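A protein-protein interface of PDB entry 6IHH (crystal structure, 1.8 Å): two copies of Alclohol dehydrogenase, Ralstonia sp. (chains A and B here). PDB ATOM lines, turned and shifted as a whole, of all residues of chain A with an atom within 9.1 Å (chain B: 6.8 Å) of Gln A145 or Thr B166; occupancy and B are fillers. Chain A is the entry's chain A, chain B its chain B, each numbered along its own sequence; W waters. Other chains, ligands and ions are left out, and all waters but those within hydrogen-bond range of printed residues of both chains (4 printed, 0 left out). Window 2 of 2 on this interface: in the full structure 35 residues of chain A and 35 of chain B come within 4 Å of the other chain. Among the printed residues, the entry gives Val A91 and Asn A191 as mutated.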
ATOM      1  N   VAL A  91      10.773   0.903 -34.313  1.00  0.00           N
ATOM      2  CA  VAL A  91      11.015   1.678 -33.110  1.00  0.00           C
ATOM      3  C   VAL A  91      12.524   1.741 -32.876  1.00  0.00           C
ATOM      4  O   VAL A  91      13.227   0.732 -32.911  1.00  0.00           O
ATOM      5  CB  VAL A  91      10.251   1.124 -31.889  1.00  0.00           C
ATOM      6  CG1 VAL A  91      10.266  -0.385 -31.831  1.00  0.00           C
ATOM      7  CG2 VAL A  91      10.756   1.710 -30.575  1.00  0.00           C
ATOM      8  N   GLU A  92      13.029   2.949 -32.680  1.00  0.00           N
ATOM      9  CA  GLU A  92      14.353   3.091 -32.112  1.00  0.00           C
ATOM     10  C   GLU A  92      14.223   4.003 -30.891  1.00  0.00           C
ATOM     11  O   GLU A  92      13.692   5.092 -31.033  1.00  0.00           O
ATOM     12  CB  GLU A  92      15.275   3.718 -33.165  1.00  0.00           C
ATOM     13  CG  GLU A  92      16.684   3.947 -32.628  1.00  0.00           C
ATOM     14  CD  GLU A  92      17.722   4.528 -33.592  1.00  0.00           C
ATOM     15  OE1 GLU A  92      17.435   5.549 -34.271  1.00  0.00           O
ATOM     16  OE2 GLU A  92      18.877   4.048 -33.549  1.00  0.00           O
ATOM     17  N   GLN A  93      14.875   3.656 -29.772  1.00  0.00           N
ATOM     18  CA  GLN A  93      14.751   4.474 -28.571  1.00  0.00           C
ATOM     19  C   GLN A  93      15.885   5.491 -28.519  1.00  0.00           C
ATOM     20  O   GLN A  93      17.058   5.133 -28.679  1.00  0.00           O
ATOM     21  CB  GLN A  93      14.750   3.606 -27.314  1.00  0.00           C
ATOM     22  CG  GLN A  93      13.620   2.579 -27.320  1.00  0.00           C
ATOM     23  CD  GLN A  93      13.614   1.809 -26.028  1.00  0.00           C
ATOM     24  OE1 GLN A  93      13.973   2.333 -24.976  1.00  0.00           O
ATOM     25  NE2 GLN A  93      13.174   0.565 -26.105  1.00  0.00           N
ATOM     26  N   LYS A  94      15.509   6.751 -28.285  1.00  0.00           N
ATOM     27  CA  LYS A  94      16.434   7.831 -27.935  1.00  0.00           C
ATOM     28  C   LYS A  94      15.677   8.765 -26.991  1.00  0.00           C
ATOM     29  O   LYS A  94      14.533   9.121 -27.279  1.00  0.00           O
ATOM     30  CB  LYS A  94      16.812   8.639 -29.189  1.00  0.00           C
ATOM     31  CG  LYS A  94      17.678   7.916 -30.232  1.00  0.00           C
ATOM     32  CD  LYS A  94      19.075   7.514 -29.728  1.00  0.00           C
ATOM     33  CE  LYS A  94      19.893   6.778 -30.772  1.00  0.00           C
ATOM     34  NZ  LYS A  94      20.963   5.975 -30.131  1.00  0.00           N
ATOM     35  N   THR A  95      16.351   9.275 -25.958  1.00  0.00           N
ATOM     36  CA  THR A  95      15.749  10.331 -25.155  1.00  0.00           C
ATOM     37  C   THR A  95      15.782  11.637 -25.942  1.00  0.00           C
ATOM     38  O   THR A  95      16.542  11.759 -26.904  1.00  0.00           O
ATOM     39  CB  THR A  95      16.478  10.496 -23.816  1.00  0.00           C
ATOM     40  OG1 THR A  95      17.806  10.826 -24.215  1.00  0.00           O
ATOM     41  CG2 THR A  95      16.536   9.188 -23.058  1.00  0.00           C
ATOM     42  N   LEU A  96      15.133  12.665 -25.379  1.00  0.00           N
ATOM     43  CA  LEU A  96      15.065  13.944 -26.065  1.00  0.00           C
ATOM     44  C   LEU A  96      16.507  14.405 -26.275  1.00  0.00           C
ATOM     45  O   LEU A  96      16.845  14.951 -27.307  1.00  0.00           O
ATOM     46  CB  LEU A  96      14.349  14.949 -25.152  1.00  0.00           C
ATOM     47  CG  LEU A  96      14.391  16.401 -25.660  1.00  0.00           C
ATOM     48  CD1 LEU A  96      13.956  16.435 -27.128  1.00  0.00           C
ATOM     49  CD2 LEU A  96      13.453  17.270 -24.832  1.00  0.00           C
ATOM     50  N   GLU A  97      17.335  14.245 -25.236  1.00  0.00           N
ATOM     51  CA  GLU A  97      18.671  14.812 -25.317  1.00  0.00           C
ATOM     52  C   GLU A  97      19.521  14.068 -26.359  1.00  0.00           C
ATOM     53  O   GLU A  97      20.452  14.642 -26.903  1.00  0.00           O
ATOM     54  CB  GLU A  97      19.328  14.913 -23.937  1.00  0.00           C
ATOM     55  CG  GLU A  97      19.703  13.566 -23.354  1.00  0.00           C
ATOM     56  CD  GLU A  97      21.122  13.454 -22.814  1.00  0.00           C
ATOM     57  OE1 GLU A  97      21.698  14.500 -22.425  1.00  0.00           O
ATOM     58  OE2 GLU A  97      21.655  12.317 -22.791  1.00  0.00           O
ATOM     59  N   GLU A  98      19.193  12.807 -26.674  1.00  0.00           N
ATOM     60  CA  GLU A  98      19.969  12.009 -27.620  1.00  0.00           C
ATOM     61  C   GLU A  98      19.442  12.122 -29.059  1.00  0.00           C
ATOM     62  O   GLU A  98      20.069  11.616 -29.993  1.00  0.00           O
ATOM     63  CB  GLU A  98      19.864  10.519 -27.278  1.00  0.00           C
ATOM     64  CG  GLU A  98      20.435  10.132 -25.941  1.00  0.00           C
ATOM     65  CD  GLU A  98      20.157   8.697 -25.492  1.00  0.00           C
ATOM     66  OE1 GLU A  98      19.030   8.097 -25.770  1.00  0.00           O
ATOM     67  OE2 GLU A  98      21.028   8.198 -24.776  1.00  0.00           O
ATOM     68  N   ALA A 139       1.814   3.535 -27.761  1.00  0.00           N
ATOM     69  CA  ALA A 139       2.805   4.572 -27.430  1.00  0.00           C
ATOM     70  C   ALA A 139       2.230   5.930 -27.831  1.00  0.00           C
ATOM     71  O   ALA A 139       2.626   6.969 -27.313  1.00  0.00           O
ATOM     72  CB  ALA A 139       4.082   4.322 -28.208  1.00  0.00           C
ATOM     73  N   LEU A 142       0.764   7.409 -24.637  1.00  0.00           N
ATOM     74  CA  LEU A 142       1.538   7.281 -23.409  1.00  0.00           C
ATOM     75  C   LEU A 142       2.771   8.173 -23.449  1.00  0.00           C
ATOM     76  O   LEU A 142       3.131   8.755 -24.480  1.00  0.00           O
ATOM     77  CB  LEU A 142       1.942   5.824 -23.164  1.00  0.00           C
ATOM     78  CG  LEU A 142       0.760   4.848 -23.102  1.00  0.00           C
ATOM     79  CD1 LEU A 142       1.266   3.397 -23.078  1.00  0.00           C
ATOM     80  CD2 LEU A 142      -0.090   5.155 -21.881  1.00  0.00           C
ATOM     81  N   GLY A 143       3.413   8.260 -22.284  1.00  0.00           N
ATOM     82  CA  GLY A 143       4.668   8.989 -22.169  1.00  0.00           C
ATOM     83  C   GLY A 143       5.776   8.033 -21.744  1.00  0.00           C
ATOM     84  O   GLY A 143       6.124   7.956 -20.558  1.00  0.00           O
ATOM     85  N   LEU A 144       6.260   7.243 -22.716  1.00  0.00           N
ATOM     86  CA  LEU A 144       7.233   6.196 -22.436  1.00  0.00           C
ATOM     87  C   LEU A 144       8.630   6.798 -22.567  1.00  0.00           C
ATOM     88  O   LEU A 144       8.977   7.366 -23.592  1.00  0.00           O
ATOM     89  CB  LEU A 144       7.012   5.087 -23.471  1.00  0.00           C
ATOM     90  CG  LEU A 144       5.604   4.485 -23.455  1.00  0.00           C
ATOM     91  CD1 LEU A 144       5.436   3.478 -24.594  1.00  0.00           C
ATOM     92  CD2 LEU A 144       5.314   3.792 -22.116  1.00  0.00           C
ATOM     93  N   GLN A 145       9.462   6.566 -21.546  1.00  0.00           N
ATOM     94  CA  GLN A 145      10.870   6.941 -21.592  1.00  0.00           C
ATOM     95  C   GLN A 145      11.534   6.543 -22.913  1.00  0.00           C
ATOM     96  O   GLN A 145      11.457   5.394 -23.341  1.00  0.00           O
ATOM     97  CB  GLN A 145      11.603   6.334 -20.390  1.00  0.00           C
ATOM     98  CG  GLN A 145      13.058   6.780 -20.337  1.00  0.00           C
ATOM     99  CD  GLN A 145      13.264   8.183 -19.821  1.00  0.00           C
ATOM    100  OE1 GLN A 145      12.395   8.803 -19.197  1.00  0.00           O
ATOM    101  NE2 GLN A 145      14.502   8.645 -19.937  1.00  0.00           N
ATOM    102  N   ALA A 146      12.203   7.533 -23.540  1.00  0.00           N
ATOM    103  CA  ALA A 146      13.085   7.377 -24.702  1.00  0.00           C
ATOM    104  C   ALA A 146      12.310   6.879 -25.926  1.00  0.00           C
ATOM    105  O   ALA A 146      12.933   6.413 -26.870  1.00  0.00           O
ATOM    106  CB  ALA A 146      14.238   6.432 -24.371  1.00  0.00           C
ATOM    107  N   HIS A 147      10.988   7.113 -25.986  1.00  0.00           N
ATOM    108  CA  HIS A 147      10.226   6.781 -27.183  1.00  0.00           C
ATOM    109  C   HIS A 147       9.730   8.053 -27.862  1.00  0.00           C
ATOM    110  O   HIS A 147       8.776   8.021 -28.639  1.00  0.00           O
ATOM    111  CB  HIS A 147       9.072   5.843 -26.818  1.00  0.00           C
ATOM    112  CG  HIS A 147       9.523   4.451 -26.528  1.00  0.00           C
ATOM    113  ND1 HIS A 147      10.213   4.119 -25.358  1.00  0.00           N
ATOM    114  CD2 HIS A 147       9.339   3.293 -27.205  1.00  0.00           C
ATOM    115  CE1 HIS A 147      10.481   2.816 -25.357  1.00  0.00           C
ATOM    116  NE2 HIS A 147       9.949   2.291 -26.478  1.00  0.00           N
ATOM    117  N   ASP A 148      10.501   9.144 -27.713  1.00  0.00           N
ATOM    118  CA  ASP A 148      10.022  10.453 -28.135  1.00  0.00           C
ATOM    119  C   ASP A 148       9.479  10.393 -29.562  1.00  0.00           C
ATOM    120  O   ASP A 148       8.326  10.745 -29.809  1.00  0.00           O
ATOM    121  CB  ASP A 148      11.135  11.505 -28.031  1.00  0.00           C
ATOM    122  CG  ASP A 148      11.720  11.585 -26.636  1.00  0.00           C
ATOM    123  OD1 ASP A 148      11.958  10.540 -26.033  1.00  0.00           O
ATOM    124  OD2 ASP A 148      11.857  12.695 -26.136  1.00  0.00           O
ATOM    125  N   THR A 149      10.338  10.054 -30.536  1.00  0.00           N
ATOM    126  CA  THR A 149       9.914  10.196 -31.927  1.00  0.00           C
ATOM    127  C   THR A 149       8.906   9.117 -32.312  1.00  0.00           C
ATOM    128  O   THR A 149       7.978   9.372 -33.084  1.00  0.00           O
ATOM    129  CB  THR A 149      11.115  10.245 -32.875  1.00  0.00           C
ATOM    130  OG1 THR A 149      11.816   9.004 -32.731  1.00  0.00           O
ATOM    131  CG2 THR A 149      12.040  11.390 -32.493  1.00  0.00           C
ATOM    132  N   TYR A 150       9.111   7.905 -31.800  1.00  0.00           N
ATOM    133  CA  TYR A 150       8.260   6.796 -32.208  1.00  0.00           C
ATOM    134  C   TYR A 150       6.828   7.039 -31.724  1.00  0.00           C
ATOM    135  O   TYR A 150       5.876   6.950 -32.494  1.00  0.00           O
ATOM    136  CB  TYR A 150       8.770   5.487 -31.599  1.00  0.00           C
ATOM    137  CG  TYR A 150       7.850   4.310 -31.826  1.00  0.00           C
ATOM    138  CD1 TYR A 150       7.850   3.611 -33.025  1.00  0.00           C
ATOM    139  CD2 TYR A 150       6.996   3.871 -30.822  1.00  0.00           C
ATOM    140  CE1 TYR A 150       6.999   2.530 -33.244  1.00  0.00           C
ATOM    141  CE2 TYR A 150       6.129   2.806 -31.030  1.00  0.00           C
ATOM    142  CZ  TYR A 150       6.153   2.113 -32.225  1.00  0.00           C
ATOM    143  OH  TYR A 150       5.311   1.064 -32.428  1.00  0.00           O
ATOM    144  N   SER A 151       6.693   7.477 -30.470  1.00  0.00           N
ATOM    145  CA  SER A 151       5.362   7.708 -29.920  1.00  0.00           C
ATOM    146  C   SER A 151       4.701   8.828 -30.719  1.00  0.00           C
ATOM    147  O   SER A 151       3.481   8.824 -30.937  1.00  0.00           O
ATOM    148  CB  SER A 151       5.447   8.052 -28.454  1.00  0.00           C
ATOM    149  OG  SER A 151       5.962   6.949 -27.694  1.00  0.00           O
ATOM    150  N   ASN A 190      13.643  -4.335 -29.602  1.00  0.00           N
ATOM    151  CA  ASN A 190      14.306  -3.280 -30.355  1.00  0.00           C
ATOM    152  C   ASN A 190      15.524  -2.736 -29.608  1.00  0.00           C
ATOM    153  O   ASN A 190      16.422  -2.170 -30.234  1.00  0.00           O
ATOM    154  CB  ASN A 190      13.327  -2.155 -30.704  1.00  0.00           C
ATOM    155  CG  ASN A 190      12.888  -1.379 -29.483  1.00  0.00           C
ATOM    156  OD1 ASN A 190      13.600  -0.476 -29.043  1.00  0.00           O
ATOM    157  ND2 ASN A 190      11.728  -1.719 -28.931  1.00  0.00           N
ATOM    158  N   ASN A 191      15.523  -2.852 -28.270  1.00  0.00           N
ATOM    159  CA  ASN A 191      16.580  -2.226 -27.486  1.00  0.00           C
ATOM    160  C   ASN A 191      17.364  -3.231 -26.639  1.00  0.00           C
ATOM    161  O   ASN A 191      18.055  -2.821 -25.709  1.00  0.00           O
ATOM    162  CB  ASN A 191      16.057  -1.095 -26.596  1.00  0.00           C
ATOM    163  CG  ASN A 191      17.174  -0.236 -26.041  1.00  0.00           C
ATOM    164  OD1 ASN A 191      18.185  -0.013 -26.706  1.00  0.00           O
ATOM    165  ND2 ASN A 191      17.007   0.250 -24.822  1.00  0.00           N
ATOM    166  N   LEU B 160       4.431  14.521 -27.677  1.00  0.00           N
ATOM    167  CA  LEU B 160       5.728  14.879 -27.089  1.00  0.00           C
ATOM    168  C   LEU B 160       5.549  15.455 -25.686  1.00  0.00           C
ATOM    169  O   LEU B 160       6.436  15.292 -24.836  1.00  0.00           O
ATOM    170  CB  LEU B 160       6.452  15.879 -28.003  1.00  0.00           C
ATOM    171  CG  LEU B 160       6.961  15.250 -29.311  1.00  0.00           C
ATOM    172  CD1 LEU B 160       7.333  16.337 -30.321  1.00  0.00           C
ATOM    173  CD2 LEU B 160       8.150  14.293 -29.060  1.00  0.00           C
ATOM    174  N   ALA B 161       4.419  16.145 -25.441  1.00  0.00           N
ATOM    175  CA  ALA B 161       4.131  16.604 -24.081  1.00  0.00           C
ATOM    176  C   ALA B 161       4.080  15.437 -23.091  1.00  0.00           C
ATOM    177  O   ALA B 161       4.571  15.577 -21.964  1.00  0.00           O
ATOM    178  CB  ALA B 161       2.868  17.438 -24.003  1.00  0.00           C
ATOM    179  N   ARG B 162       3.490  14.296 -23.496  1.00  0.00           N
ATOM    180  CA  ARG B 162       3.468  13.130 -22.591  1.00  0.00           C
ATOM    181  C   ARG B 162       4.894  12.606 -22.359  1.00  0.00           C
ATOM    182  O   ARG B 162       5.294  12.306 -21.224  1.00  0.00           O
ATOM    183  CB  ARG B 162       2.604  12.006 -23.184  1.00  0.00           C
ATOM    184  CG  ARG B 162       1.201  12.455 -23.591  1.00  0.00           C
ATOM    185  CD  ARG B 162       0.448  11.209 -24.065  1.00  0.00           C
ATOM    186  NE  ARG B 162      -0.872  11.487 -24.662  1.00  0.00           N
ATOM    187  CZ  ARG B 162      -2.034  11.436 -24.032  1.00  0.00           C
ATOM    188  NH1 ARG B 162      -2.070  11.356 -22.713  1.00  0.00           N
ATOM    189  NH2 ARG B 162      -3.162  11.446 -24.733  1.00  0.00           N
ATOM    190  N   THR B 163       5.616  12.298 -23.439  1.00  0.00           N
ATOM    191  CA  THR B 163       6.954  11.734 -23.316  1.00  0.00           C
ATOM    192  C   THR B 163       7.854  12.635 -22.474  1.00  0.00           C
ATOM    193  O   THR B 163       8.623  12.134 -21.647  1.00  0.00           O
ATOM    194  CB  THR B 163       7.582  11.497 -24.687  1.00  0.00           C
ATOM    195  OG1 THR B 163       6.690  10.657 -25.419  1.00  0.00           O
ATOM    196  CG2 THR B 163       8.951  10.860 -24.626  1.00  0.00           C
ATOM    197  N   TRP B 164       7.810  13.941 -22.753  1.00  0.00           N
ATOM    198  CA  TRP B 164       8.701  14.836 -22.025  1.00  0.00           C
ATOM    199  C   TRP B 164       8.295  15.023 -20.565  1.00  0.00           C
ATOM    200  O   TRP B 164       9.149  15.290 -19.723  1.00  0.00           O
ATOM    201  CB  TRP B 164       8.853  16.172 -22.764  1.00  0.00           C
ATOM    202  CG  TRP B 164       9.476  15.990 -24.120  1.00  0.00           C
ATOM    203  CD1 TRP B 164      10.292  14.979 -24.554  1.00  0.00           C
ATOM    204  CD2 TRP B 164       9.382  16.917 -25.204  1.00  0.00           C
ATOM    205  NE1 TRP B 164      10.666  15.193 -25.865  1.00  0.00           N
ATOM    206  CE2 TRP B 164      10.116  16.376 -26.286  1.00  0.00           C
ATOM    207  CE3 TRP B 164       8.702  18.131 -25.369  1.00  0.00           C
ATOM    208  CZ2 TRP B 164      10.220  17.033 -27.513  1.00  0.00           C
ATOM    209  CZ3 TRP B 164       8.817  18.786 -26.577  1.00  0.00           C
ATOM    210  CH2 TRP B 164       9.609  18.268 -27.608  1.00  0.00           C
ATOM    211  N   THR B 165       7.008  14.857 -20.249  1.00  0.00           N
ATOM    212  CA  THR B 165       6.589  14.772 -18.850  1.00  0.00           C
ATOM    213  C   THR B 165       7.367  13.657 -18.148  1.00  0.00           C
ATOM    214  O   THR B 165       7.968  13.868 -17.078  1.00  0.00           O
ATOM    215  CB  THR B 165       5.080  14.445 -18.745  1.00  0.00           C
ATOM    216  OG1 THR B 165       4.422  15.643 -19.136  1.00  0.00           O
ATOM    217  CG2 THR B 165       4.646  14.151 -17.324  1.00  0.00           C
ATOM    218  N   THR B 166       7.390  12.468 -18.777  1.00  0.00           N
ATOM    219  CA  THR B 166       8.122  11.330 -18.201  1.00  0.00           C
ATOM    220  C   THR B 166       9.625  11.625 -18.123  1.00  0.00           C
ATOM    221  O   THR B 166      10.284  11.323 -17.114  1.00  0.00           O
ATOM    222  CB  THR B 166       7.867  10.048 -19.011  1.00  0.00           C
ATOM    223  OG1 THR B 166       6.497   9.722 -18.724  1.00  0.00           O
ATOM    224  CG2 THR B 166       8.734   8.889 -18.529  1.00  0.00           C
ATOM    225  N   GLU B 167      10.187  12.213 -19.184  1.00  0.00           N
ATOM    226  CA  GLU B 167      11.644  12.369 -19.243  1.00  0.00           C
ATOM    227  C   GLU B 167      12.143  13.479 -18.324  1.00  0.00           C
ATOM    228  O   GLU B 167      13.294  13.425 -17.830  1.00  0.00           O
ATOM    229  CB  GLU B 167      12.113  12.607 -20.679  1.00  0.00           C
ATOM    230  CG  GLU B 167      11.983  11.349 -21.536  1.00  0.00           C
ATOM    231  CD  GLU B 167      12.657  11.404 -22.895  1.00  0.00           C
ATOM    232  OE1 GLU B 167      13.387  12.401 -23.190  1.00  0.00           O
ATOM    233  OE2 GLU B 167      12.475  10.432 -23.652  1.00  0.00           O
ATOM    234  N   LEU B 168      11.310  14.502 -18.130  1.00  0.00           N
ATOM    235  CA  LEU B 168      11.767  15.671 -17.379  1.00  0.00           C
ATOM    236  C   LEU B 168      11.196  15.731 -15.953  1.00  0.00           C
ATOM    237  O   LEU B 168      11.561  16.626 -15.188  1.00  0.00           O
ATOM    238  CB  LEU B 168      11.439  16.942 -18.181  1.00  0.00           C
ATOM    239  CG  LEU B 168      12.003  17.018 -19.604  1.00  0.00           C
ATOM    240  CD1 LEU B 168      11.604  18.351 -20.267  1.00  0.00           C
ATOM    241  CD2 LEU B 168      13.540  16.895 -19.600  1.00  0.00           C
ATOM    242  N   LYS B 169      10.499  14.684 -15.496  1.00  0.00           N
ATOM    243  CA  LYS B 169       9.871  14.787 -14.183  1.00  0.00           C
ATOM    244  C   LYS B 169      10.941  14.847 -13.090  1.00  0.00           C
ATOM    245  O   LYS B 169      10.722  15.416 -12.024  1.00  0.00           O
ATOM    246  CB  LYS B 169       8.926  13.597 -13.976  1.00  0.00           C
ATOM    247  CG  LYS B 169       9.617  12.233 -14.001  1.00  0.00           C
ATOM    248  CD  LYS B 169       8.653  11.057 -13.982  1.00  0.00           C
ATOM    249  CE  LYS B 169       9.381   9.729 -14.056  1.00  0.00           C
ATOM    250  NZ  LYS B 169       8.419   8.648 -14.343  1.00  0.00           N
ATOM    251  N   GLY B 170      12.114  14.260 -13.361  1.00  0.00           N
ATOM    252  CA  GLY B 170      13.136  14.210 -12.323  1.00  0.00           C
ATOM    253  C   GLY B 170      13.670  15.608 -12.030  1.00  0.00           C
ATOM    254  O   GLY B 170      14.224  15.851 -10.951  1.00  0.00           O
HETATM  255  O   HOH W   1      12.056   8.863 -16.652  1.00  0.00           O
HETATM  256  O   HOH W   2       5.759   8.104 -25.370  1.00  0.00           O
HETATM  257  O   HOH W   3       6.311  11.599 -27.945  1.00  0.00           O
HETATM  258  O   HOH W   4      15.125  11.266 -18.843  1.00  0.00           O
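The side-chain carboxylate (OD2) of Asp A148 sits at hydrogen-bond distance from the indole nitrogen (NE1) of Trp B164, 2.8 Å away. OD1 of Asp A148 sits close to OE2 of Glu B167 (2.4 Å). O of Gly A143 is in hydrogen-bond range of OG1 of Thr B166, at 2.6 Å. The backbone NH (N) of Leu A96 is in hydrogen-bond range of the side-chain carboxylate (OE1) of Glu B167 (2.8 Å). The backbone NH (N) of Ala A146 is in hydrogen-bond range of the side-chain carboxylate (OE2) of Glu B167.
The backbone NH (N) of Leu A96 is in hydrogen-bond range of the side-chain carboxylate (OD2) of Asp A148, 3.4 Å away. The backbone NH (N) of Lys A94 lies within hydrogen-bond range of the backbone carbonyl oxygen (O) of Ala A146 (3.0 Å). N of Thr A95 lies within hydrogen-bond range of OE1 of Glu A98, 2.9 Å away. The backbone carbonyl oxygen of Gln A145 lies within hydrogen-bond range of a ring nitrogen (ND1) of His A147 (2.7 Å).
Among the printed residues, merely in contact across the chains: Thr A95 with Glu B167 (3.6 Å), Leu A96 with Trp B164 (3.6 Å), Leu A142 with Arg B162 (3.5 Å), Gly A143 with Arg B162 (3.5 Å), Gly A143 with Thr B163 (3.7 Å), Leu A144 with Thr B163 (3.6 Å), Gln A145 with Thr B166 (3.7 Å), Gln A145 with Glu B167 (3.5 Å), Asp A148 with Leu B160 (3.6 Å) and Asp A148 with Thr B163 (3.3 Å).
Of chain B, only Thr B166 (3.7 Å) and Glu B167 (3.5 Å) come within 4 Å of Gln A145. Thr B166 touches just these residues of chain A: Gly A143 (2.6 Å) and Gln A145 (3.7 Å). No residue of chain A comes within 4 Å of Thr B165. Of the printed residues of chain B, Ala A146 touches Glu B167 (2.9 Å). Of the printed residues of chain B, Asp A148 touches Leu B160, Thr B163, Trp B164 and Glu B167. Of the printed residues of chain A, Arg B162 touches Leu A142 (3.5 Å) and Gly A143 (3.5 Å). Printed residues of chain B within 4 Å of Leu A96: Trp B164 and Glu B167. Of the printed residues of chain B, Gly A143 touches Arg B162, Thr B163 and Thr B166. His A147 touches none of the printed residues of chain B. Asn A190 touches none of the printed residues of chain B. The nearest residue of chain B that does not touch Gln A145 is Thr B163 (5.3 Å). The nearest printed residue of chain B that does not touch Thr A95 is Trp B164 (6.2 Å).
Printed residues of chain B that touch a printed residue of chain A: Leu B160, Arg B162, Thr B163, Trp B164, Thr B166 and Glu B167. Hydrophobic or aromatic side chains of chain B within 4 Å of the printed part of chain A: Leu B160 and Trp B164. Among the printed residues, no Asp or Glu carboxylate lies within 4 Å of a Lys or Arg side-chain nitrogen of the other chain.
No position is printed for both chains.
Water W1 bridges the side-chain amide oxygen of Gln A145 (2.6 Å) and the backbone carbonyl oxygen of Thr B166 (3.1 Å). Water W2 lies within hydrogen-bond range of OG of Ser A151, OG1 of Thr B163, N of Leu A144 and O of Leu A142. Water W3 lies within hydrogen-bond range of OG1 of Thr B163 (2.7 Å), O of Asp A148 (2.9 Å) and N of Leu B160 (3.5 Å). Water W4 bridges NE2 of Gln A145 (2.9 Å) and O of Glu B167 (3.0 Å).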
